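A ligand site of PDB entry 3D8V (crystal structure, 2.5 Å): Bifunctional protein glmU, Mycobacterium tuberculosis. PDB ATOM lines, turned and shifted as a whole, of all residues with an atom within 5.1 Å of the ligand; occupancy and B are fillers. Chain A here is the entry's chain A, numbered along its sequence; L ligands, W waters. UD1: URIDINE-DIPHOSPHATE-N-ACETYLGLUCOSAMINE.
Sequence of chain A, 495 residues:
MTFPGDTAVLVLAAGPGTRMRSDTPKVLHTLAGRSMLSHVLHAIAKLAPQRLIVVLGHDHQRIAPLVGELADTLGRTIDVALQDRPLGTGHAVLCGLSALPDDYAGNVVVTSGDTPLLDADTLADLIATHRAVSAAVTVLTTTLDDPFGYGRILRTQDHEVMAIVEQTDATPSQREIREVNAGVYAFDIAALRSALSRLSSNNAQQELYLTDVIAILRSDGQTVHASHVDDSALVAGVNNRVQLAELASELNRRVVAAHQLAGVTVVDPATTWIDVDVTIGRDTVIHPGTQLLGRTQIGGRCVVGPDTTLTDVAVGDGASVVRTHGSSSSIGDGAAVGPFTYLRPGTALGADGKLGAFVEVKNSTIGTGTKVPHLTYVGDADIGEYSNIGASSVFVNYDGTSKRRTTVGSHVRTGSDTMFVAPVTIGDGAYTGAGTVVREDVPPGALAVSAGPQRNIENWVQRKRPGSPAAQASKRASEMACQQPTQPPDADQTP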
ATOM      1  N   LEU A  12      16.595 -24.541 -26.805  1.00  0.00           N
ATOM      2  CA  LEU A  12      16.448 -23.753 -25.593  1.00  0.00           C
ATOM      3  C   LEU A  12      17.618 -24.003 -24.658  1.00  0.00           C
ATOM      4  O   LEU A  12      17.887 -25.144 -24.285  1.00  0.00           O
ATOM      5  CB  LEU A  12      15.138 -24.101 -24.900  1.00  0.00           C
ATOM      6  CG  LEU A  12      13.905 -24.167 -25.800  1.00  0.00           C
ATOM      7  CD1 LEU A  12      12.659 -24.316 -24.956  1.00  0.00           C
ATOM      8  CD2 LEU A  12      13.810 -22.921 -26.658  1.00  0.00           C
ATOM      9  N   ALA A  13      18.291 -22.933 -24.255  1.00  0.00           N
ATOM     10  CA  ALA A  13      19.443 -23.061 -23.364  1.00  0.00           C
ATOM     11  C   ALA A  13      19.574 -21.878 -22.418  1.00  0.00           C
ATOM     12  O   ALA A  13      20.661 -21.613 -21.887  1.00  0.00           O
ATOM     13  CB  ALA A  13      20.720 -23.227 -24.177  1.00  0.00           C
ATOM     14  N   ALA A  14      18.469 -21.178 -22.187  1.00  0.00           N
ATOM     15  CA  ALA A  14      18.516 -19.893 -21.480  1.00  0.00           C
ATOM     16  C   ALA A  14      18.062 -19.987 -20.034  1.00  0.00           C
ATOM     17  O   ALA A  14      17.954 -18.968 -19.343  1.00  0.00           O
ATOM     18  CB  ALA A  14      17.709 -18.838 -22.223  1.00  0.00           C
ATOM     19  N   GLY A  15      17.796 -21.197 -19.564  1.00  0.00           N
ATOM     20  CA  GLY A  15      17.410 -21.400 -18.183  1.00  0.00           C
ATOM     21  C   GLY A  15      18.588 -21.133 -17.280  1.00  0.00           C
ATOM     22  O   GLY A  15      19.745 -21.208 -17.719  1.00  0.00           O
ATOM     23  N   ARG A  19      19.578 -25.871 -10.133  1.00  0.00           N
ATOM     24  CA  ARG A  19      19.734 -27.175  -9.490  1.00  0.00           C
ATOM     25  C   ARG A  19      21.103 -27.830  -9.673  1.00  0.00           C
ATOM     26  O   ARG A  19      21.382 -28.852  -9.046  1.00  0.00           O
ATOM     27  CB  ARG A  19      18.629 -28.140  -9.914  1.00  0.00           C
ATOM     28  CG  ARG A  19      17.332 -27.912  -9.162  1.00  0.00           C
ATOM     29  CD  ARG A  19      16.184 -28.618  -9.836  1.00  0.00           C
ATOM     30  NE  ARG A  19      15.990 -28.104 -11.180  1.00  0.00           N
ATOM     31  CZ  ARG A  19      15.205 -28.662 -12.086  1.00  0.00           C
ATOM     32  NH1 ARG A  19      14.531 -29.761 -11.781  1.00  0.00           N
ATOM     33  NH2 ARG A  19      15.082 -28.122 -13.288  1.00  0.00           N
ATOM     34  N   LYS A  26      25.097 -24.589 -16.961  1.00  0.00           N
ATOM     35  CA  LYS A  26      24.720 -25.991 -17.060  1.00  0.00           C
ATOM     36  C   LYS A  26      25.225 -26.642 -18.355  1.00  0.00           C
ATOM     37  O   LYS A  26      25.934 -27.648 -18.322  1.00  0.00           O
ATOM     38  CB  LYS A  26      23.202 -26.137 -16.936  1.00  0.00           C
ATOM     39  CG  LYS A  26      22.740 -27.578 -16.843  1.00  0.00           C
ATOM     40  CD  LYS A  26      21.375 -27.771 -17.485  1.00  0.00           C
ATOM     41  CE  LYS A  26      20.271 -27.133 -16.662  1.00  0.00           C
ATOM     42  NZ  LYS A  26      18.929 -27.547 -17.161  1.00  0.00           N
ATOM     43  N   VAL A  55      18.845 -20.383 -28.215  1.00  0.00           N
ATOM     44  CA  VAL A  55      18.368 -19.379 -27.273  1.00  0.00           C
ATOM     45  C   VAL A  55      19.224 -19.383 -26.007  1.00  0.00           C
ATOM     46  O   VAL A  55      19.352 -20.399 -25.345  1.00  0.00           O
ATOM     47  CB  VAL A  55      16.918 -19.663 -26.872  1.00  0.00           C
ATOM     48  CG1 VAL A  55      16.343 -18.503 -26.082  1.00  0.00           C
ATOM     49  CG2 VAL A  55      16.081 -19.968 -28.112  1.00  0.00           C
ATOM     50  N   GLN A  83      17.278 -14.193 -24.600  1.00  0.00           N
ATOM     51  CA  GLN A  83      16.131 -14.113 -23.710  1.00  0.00           C
ATOM     52  C   GLN A  83      16.628 -13.596 -22.377  1.00  0.00           C
ATOM     53  O   GLN A  83      17.067 -14.377 -21.528  1.00  0.00           O
ATOM     54  CB  GLN A  83      15.473 -15.481 -23.535  1.00  0.00           C
ATOM     55  CG  GLN A  83      14.320 -15.500 -22.539  1.00  0.00           C
ATOM     56  CD  GLN A  83      13.931 -16.904 -22.085  1.00  0.00           C
ATOM     57  OE1 GLN A  83      14.764 -17.815 -22.084  1.00  0.00           O
ATOM     58  NE2 GLN A  83      12.680 -17.069 -21.698  1.00  0.00           N
ATOM     59  N   ARG A  85      15.518 -12.573 -19.526  1.00  0.00           N
ATOM     60  CA  ARG A  85      15.050 -13.207 -18.305  1.00  0.00           C
ATOM     61  C   ARG A  85      14.259 -14.458 -18.612  1.00  0.00           C
ATOM     62  O   ARG A  85      13.479 -14.484 -19.564  1.00  0.00           O
ATOM     63  CB  ARG A  85      14.226 -12.229 -17.463  1.00  0.00           C
ATOM     64  CG  ARG A  85      15.058 -11.190 -16.740  1.00  0.00           C
ATOM     65  CD  ARG A  85      14.300  -9.882 -16.616  1.00  0.00           C
ATOM     66  NE  ARG A  85      13.470  -9.665 -17.795  1.00  0.00           N
ATOM     67  CZ  ARG A  85      12.136  -9.604 -17.772  1.00  0.00           C
ATOM     68  NH1 ARG A  85      11.487  -9.735 -16.624  1.00  0.00           N
ATOM     69  NH2 ARG A  85      11.471  -9.398 -18.907  1.00  0.00           N
ATOM     70  N   PRO A  86      14.476 -15.511 -17.820  1.00  0.00           N
ATOM     71  CA  PRO A  86      13.816 -16.801 -17.999  1.00  0.00           C
ATOM     72  C   PRO A  86      12.357 -16.710 -17.588  1.00  0.00           C
ATOM     73  O   PRO A  86      12.010 -17.030 -16.453  1.00  0.00           O
ATOM     74  CB  PRO A  86      14.573 -17.700 -17.011  1.00  0.00           C
ATOM     75  CG  PRO A  86      15.034 -16.739 -15.961  1.00  0.00           C
ATOM     76  CD  PRO A  86      15.495 -15.568 -16.761  1.00  0.00           C
ATOM     77  N   LEU A  87      11.515 -16.259 -18.502  1.00  0.00           N
ATOM     78  CA  LEU A  87      10.106 -16.080 -18.198  1.00  0.00           C
ATOM     79  C   LEU A  87       9.338 -17.350 -18.475  1.00  0.00           C
ATOM     80  O   LEU A  87       8.132 -17.423 -18.249  1.00  0.00           O
ATOM     81  CB  LEU A  87       9.516 -14.917 -19.001  1.00  0.00           C
ATOM     82  CG  LEU A  87      10.179 -13.579 -18.697  1.00  0.00           C
ATOM     83  CD1 LEU A  87       9.616 -12.505 -19.609  1.00  0.00           C
ATOM     84  CD2 LEU A  87       9.975 -13.217 -17.244  1.00  0.00           C
ATOM     85  N   GLY A  88      10.047 -18.361 -18.974  1.00  0.00           N
ATOM     86  CA  GLY A  88       9.439 -19.638 -19.262  1.00  0.00           C
ATOM     87  C   GLY A  88       9.888 -20.239 -20.559  1.00  0.00           C
ATOM     88  O   GLY A  88      10.493 -19.571 -21.408  1.00  0.00           O
ATOM     89  N   THR A  89       9.601 -21.521 -20.724  1.00  0.00           N
ATOM     90  CA  THR A  89      10.020 -22.246 -21.912  1.00  0.00           C
ATOM     91  C   THR A  89       9.301 -21.694 -23.132  1.00  0.00           C
ATOM     92  O   THR A  89       9.909 -21.490 -24.180  1.00  0.00           O
ATOM     93  CB  THR A  89       9.767 -23.757 -21.752  1.00  0.00           C
ATOM     94  OG1 THR A  89       8.389 -23.969 -21.419  1.00  0.00           O
ATOM     95  CG2 THR A  89      10.636 -24.315 -20.640  1.00  0.00           C
ATOM     96  N   ALA A  92      10.841 -18.548 -24.129  1.00  0.00           N
ATOM     97  CA  ALA A  92      12.123 -18.845 -24.772  1.00  0.00           C
ATOM     98  C   ALA A  92      11.918 -19.192 -26.241  1.00  0.00           C
ATOM     99  O   ALA A  92      12.725 -18.807 -27.088  1.00  0.00           O
ATOM    100  CB  ALA A  92      12.832 -19.992 -24.046  1.00  0.00           C
ATOM    101  N   SER A 112      16.110 -29.186 -26.249  1.00  0.00           N
ATOM    102  CA  SER A 112      16.818 -28.537 -25.150  1.00  0.00           C
ATOM    103  C   SER A 112      18.327 -28.703 -25.272  1.00  0.00           C
ATOM    104  O   SER A 112      18.822 -29.615 -25.950  1.00  0.00           O
ATOM    105  CB  SER A 112      16.323 -29.088 -23.807  1.00  0.00           C
ATOM    106  OG  SER A 112      16.838 -28.333 -22.738  1.00  0.00           O
ATOM    107  N   GLY A 113      19.073 -27.819 -24.611  1.00  0.00           N
ATOM    108  CA  GLY A 113      20.526 -27.889 -24.652  1.00  0.00           C
ATOM    109  C   GLY A 113      21.103 -28.865 -23.635  1.00  0.00           C
ATOM    110  O   GLY A 113      22.328 -29.030 -23.559  1.00  0.00           O
ATOM    111  N   ASP A 114      20.230 -29.512 -22.862  1.00  0.00           N
ATOM    112  CA  ASP A 114      20.654 -30.384 -21.763  1.00  0.00           C
ATOM    113  C   ASP A 114      20.255 -31.860 -21.953  1.00  0.00           C
ATOM    114  O   ASP A 114      20.035 -32.578 -20.969  1.00  0.00           O
ATOM    115  CB  ASP A 114      20.120 -29.835 -20.427  1.00  0.00           C
ATOM    116  CG  ASP A 114      18.604 -29.814 -20.354  1.00  0.00           C
ATOM    117  OD1 ASP A 114      17.955 -30.373 -21.266  1.00  0.00           O
ATOM    118  OD2 ASP A 114      18.062 -29.234 -19.383  1.00  0.00           O
ATOM    119  N   GLY A 149       9.254 -34.717 -11.357  1.00  0.00           N
ATOM    120  CA  GLY A 149       9.860 -33.506 -11.880  1.00  0.00           C
ATOM    121  C   GLY A 149       9.530 -33.180 -13.318  1.00  0.00           C
ATOM    122  O   GLY A 149       9.759 -32.063 -13.782  1.00  0.00           O
ATOM    123  N   TYR A 150       8.983 -34.153 -14.046  1.00  0.00           N
ATOM    124  CA  TYR A 150       8.743 -33.971 -15.464  1.00  0.00           C
ATOM    125  C   TYR A 150       7.266 -33.788 -15.748  1.00  0.00           C
ATOM    126  O   TYR A 150       6.425 -34.051 -14.896  1.00  0.00           O
ATOM    127  CB  TYR A 150       9.328 -35.129 -16.253  1.00  0.00           C
ATOM    128  CG  TYR A 150      10.830 -35.187 -16.110  1.00  0.00           C
ATOM    129  CD1 TYR A 150      11.443 -36.188 -15.353  1.00  0.00           C
ATOM    130  CD2 TYR A 150      11.631 -34.211 -16.685  1.00  0.00           C
ATOM    131  CE1 TYR A 150      12.834 -36.221 -15.216  1.00  0.00           C
ATOM    132  CE2 TYR A 150      12.998 -34.231 -16.556  1.00  0.00           C
ATOM    133  CZ  TYR A 150      13.605 -35.239 -15.819  1.00  0.00           C
ATOM    134  OH  TYR A 150      14.978 -35.237 -15.694  1.00  0.00           O
ATOM    135  N   GLY A 151       6.971 -33.309 -16.946  1.00  0.00           N
ATOM    136  CA  GLY A 151       5.593 -33.067 -17.331  1.00  0.00           C
ATOM    137  C   GLY A 151       4.839 -34.353 -17.602  1.00  0.00           C
ATOM    138  O   GLY A 151       5.274 -35.187 -18.404  1.00  0.00           O
ATOM    139  N   ILE A 164      -0.325 -31.494 -21.377  1.00  0.00           N
ATOM    140  CA  ILE A 164       0.807 -31.825 -20.544  1.00  0.00           C
ATOM    141  C   ILE A 164       0.695 -31.048 -19.250  1.00  0.00           C
ATOM    142  O   ILE A 164       0.431 -29.845 -19.271  1.00  0.00           O
ATOM    143  CB  ILE A 164       2.134 -31.442 -21.201  1.00  0.00           C
ATOM    144  CG1 ILE A 164       2.252 -32.091 -22.578  1.00  0.00           C
ATOM    145  CG2 ILE A 164       3.291 -31.821 -20.299  1.00  0.00           C
ATOM    146  CD1 ILE A 164       3.568 -31.772 -23.263  1.00  0.00           C
ATOM    147  N   GLU A 166       2.639 -29.999 -15.627  1.00  0.00           N
ATOM    148  CA  GLU A 166       3.923 -29.952 -14.943  1.00  0.00           C
ATOM    149  C   GLU A 166       3.867 -30.503 -13.520  1.00  0.00           C
ATOM    150  O   GLU A 166       2.799 -30.516 -12.907  1.00  0.00           O
ATOM    151  CB  GLU A 166       4.450 -28.521 -14.938  1.00  0.00           C
ATOM    152  CG  GLU A 166       4.721 -28.007 -16.334  1.00  0.00           C
ATOM    153  CD  GLU A 166       5.794 -28.809 -17.038  1.00  0.00           C
ATOM    154  OE1 GLU A 166       6.979 -28.691 -16.651  1.00  0.00           O
ATOM    155  OE2 GLU A 166       5.452 -29.568 -17.970  1.00  0.00           O
ATOM    156  N   ASN A 181       6.660 -35.865 -20.483  1.00  0.00           N
ATOM    157  CA  ASN A 181       7.047 -35.017 -21.595  1.00  0.00           C
ATOM    158  C   ASN A 181       8.553 -35.008 -21.739  1.00  0.00           C
ATOM    159  O   ASN A 181       9.261 -34.680 -20.791  1.00  0.00           O
ATOM    160  CB  ASN A 181       6.565 -33.599 -21.321  1.00  0.00           C
ATOM    161  CG  ASN A 181       6.933 -32.645 -22.421  1.00  0.00           C
ATOM    162  OD1 ASN A 181       7.204 -33.046 -23.548  1.00  0.00           O
ATOM    163  ND2 ASN A 181       6.961 -31.364 -22.083  1.00  0.00           N
ATOM    164  N   ALA A 182       9.040 -35.333 -22.930  1.00  0.00           N
ATOM    165  CA  ALA A 182      10.487 -35.369 -23.179  1.00  0.00           C
ATOM    166  C   ALA A 182      11.085 -34.003 -23.459  1.00  0.00           C
ATOM    167  O   ALA A 182      12.301 -33.822 -23.396  1.00  0.00           O
ATOM    168  CB  ALA A 182      10.803 -36.303 -24.335  1.00  0.00           C
ATOM    169  N   GLY A 183      10.217 -33.050 -23.801  1.00  0.00           N
ATOM    170  CA  GLY A 183      10.635 -31.689 -24.134  1.00  0.00           C
ATOM    171  C   GLY A 183      11.286 -31.587 -25.494  1.00  0.00           C
ATOM    172  O   GLY A 183      12.165 -30.737 -25.721  1.00  0.00           O
ATOM    173  N   TYR A 185      10.001 -31.302 -29.482  1.00  0.00           N
ATOM    174  CA  TYR A 185       8.775 -31.008 -30.219  1.00  0.00           C
ATOM    175  C   TYR A 185       9.006 -30.800 -31.713  1.00  0.00           C
ATOM    176  O   TYR A 185      10.117 -30.480 -32.154  1.00  0.00           O
ATOM    177  CB  TYR A 185       8.134 -29.726 -29.690  1.00  0.00           C
ATOM    178  CG  TYR A 185       7.930 -29.615 -28.186  1.00  0.00           C
ATOM    179  CD1 TYR A 185       8.977 -29.267 -27.337  1.00  0.00           C
ATOM    180  CD2 TYR A 185       6.671 -29.787 -27.631  1.00  0.00           C
ATOM    181  CE1 TYR A 185       8.771 -29.131 -25.965  1.00  0.00           C
ATOM    182  CE2 TYR A 185       6.466 -29.647 -26.280  1.00  0.00           C
ATOM    183  CZ  TYR A 185       7.512 -29.325 -25.446  1.00  0.00           C
ATOM    184  OH  TYR A 185       7.269 -29.195 -24.100  1.00  0.00           O
ATOM    185  N   TYR A 209       4.497 -21.431 -19.923  1.00  0.00           N
ATOM    186  CA  TYR A 209       4.797 -22.848 -20.156  1.00  0.00           C
ATOM    187  C   TYR A 209       4.646 -23.244 -21.614  1.00  0.00           C
ATOM    188  O   TYR A 209       3.540 -23.328 -22.130  1.00  0.00           O
ATOM    189  CB  TYR A 209       3.839 -23.730 -19.350  1.00  0.00           C
ATOM    190  CG  TYR A 209       4.014 -23.751 -17.838  1.00  0.00           C
ATOM    191  CD1 TYR A 209       5.135 -23.188 -17.228  1.00  0.00           C
ATOM    192  CD2 TYR A 209       3.087 -24.401 -17.032  1.00  0.00           C
ATOM    193  CE1 TYR A 209       5.281 -23.240 -15.839  1.00  0.00           C
ATOM    194  CE2 TYR A 209       3.236 -24.459 -15.661  1.00  0.00           C
ATOM    195  CZ  TYR A 209       4.323 -23.877 -15.072  1.00  0.00           C
ATOM    196  OH  TYR A 209       4.446 -23.952 -13.703  1.00  0.00           O
ATOM    197  N   LEU A 210       5.756 -23.548 -22.287  1.00  0.00           N
ATOM    198  CA  LEU A 210       5.652 -24.036 -23.661  1.00  0.00           C
ATOM    199  C   LEU A 210       4.673 -25.211 -23.697  1.00  0.00           C
ATOM    200  O   LEU A 210       3.972 -25.397 -24.679  1.00  0.00           O
ATOM    201  CB  LEU A 210       7.012 -24.467 -24.205  1.00  0.00           C
ATOM    202  CG  LEU A 210       6.971 -25.199 -25.549  1.00  0.00           C
ATOM    203  CD1 LEU A 210       6.379 -24.325 -26.648  1.00  0.00           C
ATOM    204  CD2 LEU A 210       8.354 -25.707 -25.934  1.00  0.00           C
ATOM    205  N   THR A 211       4.632 -25.975 -22.616  1.00  0.00           N
ATOM    206  CA  THR A 211       3.754 -27.140 -22.552  1.00  0.00           C
ATOM    207  C   THR A 211       2.254 -26.829 -22.673  1.00  0.00           C
ATOM    208  O   THR A 211       1.486 -27.686 -23.115  1.00  0.00           O
ATOM    209  CB  THR A 211       3.996 -27.959 -21.270  1.00  0.00           C
ATOM    210  OG1 THR A 211       4.029 -27.068 -20.145  1.00  0.00           O
ATOM    211  CG2 THR A 211       5.316 -28.705 -21.357  1.00  0.00           C
ATOM    212  N   ASN A 239      19.282 -31.882 -15.200  1.00  0.00           N
ATOM    213  CA  ASN A 239      18.931 -30.720 -14.369  1.00  0.00           C
ATOM    214  C   ASN A 239      19.798 -30.573 -13.106  1.00  0.00           C
ATOM    215  O   ASN A 239      19.895 -29.487 -12.540  1.00  0.00           O
ATOM    216  CB  ASN A 239      17.432 -30.723 -14.026  1.00  0.00           C
ATOM    217  CG  ASN A 239      16.545 -30.366 -15.228  1.00  0.00           C
ATOM    218  OD1 ASN A 239      17.012 -29.819 -16.230  1.00  0.00           O
ATOM    219  ND2 ASN A 239      15.250 -30.676 -15.117  1.00  0.00           N
HETATM  220  C1' UD1 L   1      10.490 -28.895 -19.107  1.00  0.00           C
HETATM  221  C2' UD1 L   1       9.015 -29.087 -19.434  1.00  0.00           C
HETATM  222  C3' UD1 L   1       8.561 -30.454 -18.949  1.00  0.00           C
HETATM  223  C4' UD1 L   1       9.456 -31.521 -19.568  1.00  0.00           C
HETATM  224  C5' UD1 L   1      10.933 -31.244 -19.283  1.00  0.00           C
HETATM  225  C6' UD1 L   1      11.843 -32.256 -19.985  1.00  0.00           C
HETATM  226  C7' UD1 L   1       7.884 -26.945 -19.406  1.00  0.00           C
HETATM  227  C8' UD1 L   1       8.538 -26.755 -20.725  1.00  0.00           C
HETATM  228  N2' UD1 L   1       8.242 -28.064 -18.771  1.00  0.00           N
HETATM  229  O1' UD1 L   1      10.634 -29.027 -17.698  1.00  0.00           O
HETATM  230  O3' UD1 L   1       7.196 -30.698 -19.286  1.00  0.00           O
HETATM  231  O4' UD1 L   1       9.046 -32.795 -19.057  1.00  0.00           O
HETATM  232  O5' UD1 L   1      11.250 -29.922 -19.739  1.00  0.00           O
HETATM  233  O6' UD1 L   1      13.160 -32.201 -19.412  1.00  0.00           O
HETATM  234  O7' UD1 L   1       7.091 -26.146 -18.943  1.00  0.00           O
HETATM  235  N1  UD1 L   1      14.549 -22.713 -20.559  1.00  0.00           N
HETATM  236  C2  UD1 L   1      14.856 -21.458 -21.126  1.00  0.00           C
HETATM  237  N3  UD1 L   1      14.260 -20.354 -20.661  1.00  0.00           N
HETATM  238  C4  UD1 L   1      13.363 -20.429 -19.666  1.00  0.00           C
HETATM  239  C5  UD1 L   1      13.047 -21.654 -19.097  1.00  0.00           C
HETATM  240  C6  UD1 L   1      13.667 -22.807 -19.567  1.00  0.00           C
HETATM  241  O2  UD1 L   1      15.688 -21.393 -22.068  1.00  0.00           O
HETATM  242  O4  UD1 L   1      12.817 -19.371 -19.253  1.00  0.00           O
HETATM  243  C1B UD1 L   1      15.235 -23.883 -21.107  1.00  0.00           C
HETATM  244  C2B UD1 L   1      16.148 -24.559 -20.103  1.00  0.00           C
HETATM  245  O2' UD1 L   1      17.481 -24.038 -20.145  1.00  0.00           O
HETATM  246  C3B UD1 L   1      16.128 -25.998 -20.589  1.00  0.00           C
HETATM  247  C4B UD1 L   1      14.766 -26.160 -21.237  1.00  0.00           C
HETATM  248  O4B UD1 L   1      14.275 -24.847 -21.536  1.00  0.00           O
HETATM  249  O3B UD1 L   1      17.161 -26.154 -21.574  1.00  0.00           O
HETATM  250  C5B UD1 L   1      13.786 -26.742 -20.227  1.00  0.00           C
HETATM  251  O5B UD1 L   1      14.026 -25.933 -19.075  1.00  0.00           O
HETATM  252  PA  UD1 L   1      13.794 -26.566 -17.643  1.00  0.00           P
HETATM  253  O1A UD1 L   1      13.608 -25.486 -16.605  1.00  0.00           O
HETATM  254  O2A UD1 L   1      14.907 -27.581 -17.565  1.00  0.00           O
HETATM  255  O3A UD1 L   1      12.403 -27.312 -17.923  1.00  0.00           O
HETATM  256  PB  UD1 L   1      11.858 -28.392 -16.888  1.00  0.00           P
HETATM  257  O1B UD1 L   1      11.303 -27.672 -15.682  1.00  0.00           O
HETATM  258  O2B UD1 L   1      12.903 -29.495 -16.728  1.00  0.00           O
HETATM  259  O   HOH W   1      15.613 -30.038 -18.587  1.00  0.00           O
HETATM  260  O   HOH W   2      20.801 -24.072 -19.727  1.00  0.00           O
HETATM  261  O   HOH W   3       8.618 -27.112 -15.255  1.00  0.00           O
HETATM  262  O   HOH W   4       9.436 -28.238 -22.998  1.00  0.00           O
HETATM  263  O   HOH W   5      18.253 -24.666 -16.950  1.00  0.00           O
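The side-chain amide oxygen (OD1) of Asn 181 sits at hydrogen-bond distance from the backbone NH (N) of Gly 183.
The side-chain hydroxyl (OG) of Ser 112 sits at hydrogen-bond distance from the side-chain carboxylate (OD1) of Asp 114 (2.8 Å).
OD1 of Asn 239 lies close to OD2 of Asp 114 (3.4 Å).
The side-chain amide nitrogen (ND2) of Asn 239 lies close to the guanidinium group (NH2) of Arg 19 (3.1 Å).
The side-chain hydroxyl of Tyr 185 lies within hydrogen-bond range of the side-chain amide nitrogen of Asn 181, 3.0 Å away.
The backbone carbonyl oxygen (O) of Val 55 lies within hydrogen-bond range of the backbone NH (N) of Ala 13 (3.0 Å).
The side-chain carboxylate (OD2) of Asp 114 is in salt-bridge range of the side-chain amino group (NZ) of Lys 26 (2.9 Å).
The backbone NH (N) of Ala 14 is in hydrogen-bond range of the backbone carbonyl oxygen (O) of Val 55.
An oxygen (O3') of the ligand lies within hydrogen-bond range of the side-chain carboxylate (OE2) of Glu 166 (2.5 Å).
N3 of the ligand sits at hydrogen-bond distance from OE1 of Gln 83.
An oxygen (O3') of the ligand lies within hydrogen-bond range of the side-chain amide nitrogen (ND2) of Asn 181.
The side-chain amide nitrogen (ND2) of Asn 239 lies within hydrogen-bond range of an oxygen (O2B) of the ligand (3.1 Å).
The backbone NH (N) of Gly 15 sits at hydrogen-bond distance from an oxygen (O2') of the ligand.
OG of Ser 112 sits at hydrogen-bond distance from O3B of the ligand.
An oxygen (O4) of the ligand lies within hydrogen-bond range of the backbone NH (N) of Leu 87, 3.5 Å away.
N of Ala 14 sits at hydrogen-bond distance from O2 of the ligand.
O of Leu 12 lies within hydrogen-bond range of O3B of the ligand, at 3.0 Å.
An oxygen (O7') of the ligand sits at hydrogen-bond distance from the side-chain hydroxyl of Thr 211, 3.4 Å away.
N of Gly 88 lies within hydrogen-bond range of O4 of the ligand (3.0 Å).
O of Asn 181 sits at hydrogen-bond distance from O4' of the ligand, 2.6 Å away.
The backbone NH (N) of Gly 151 sits at hydrogen-bond distance from an oxygen (O4') of the ligand, 3.0 Å away.
Residues that only touch the ligand: Thr 89 (2.9 Å), Pro 86 (3.0 Å), Tyr 150 (3.5 Å), Ala 92 (3.7 Å), Ala 13 (3.7 Å), Ala 182 (3.8 Å), Asp 114 (3.9 Å), Tyr 209 (3.9 Å) and Gly 113 (3.96 Å).
Water W1 lies within hydrogen-bond range of the side-chain carboxylate of Asp 114 (2.7 Å), the side-chain amide oxygen of Asn 239 (2.7 Å) and an oxygen (O2A) of the ligand (2.8 Å).
Water W3 lies within hydrogen-bond range of the side-chain carboxylate of Glu 166 (2.7 Å) and an oxygen (O1B) of the ligand (2.8 Å).
Water W5 lies within hydrogen-bond range of NZ of Lys 26 (3.0 Å) and O2' of the ligand (3.3 Å).
Water W2 lies within hydrogen-bond range of O of Ala 13 (3.3 Å) and O2' of the ligand (3.3 Å).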
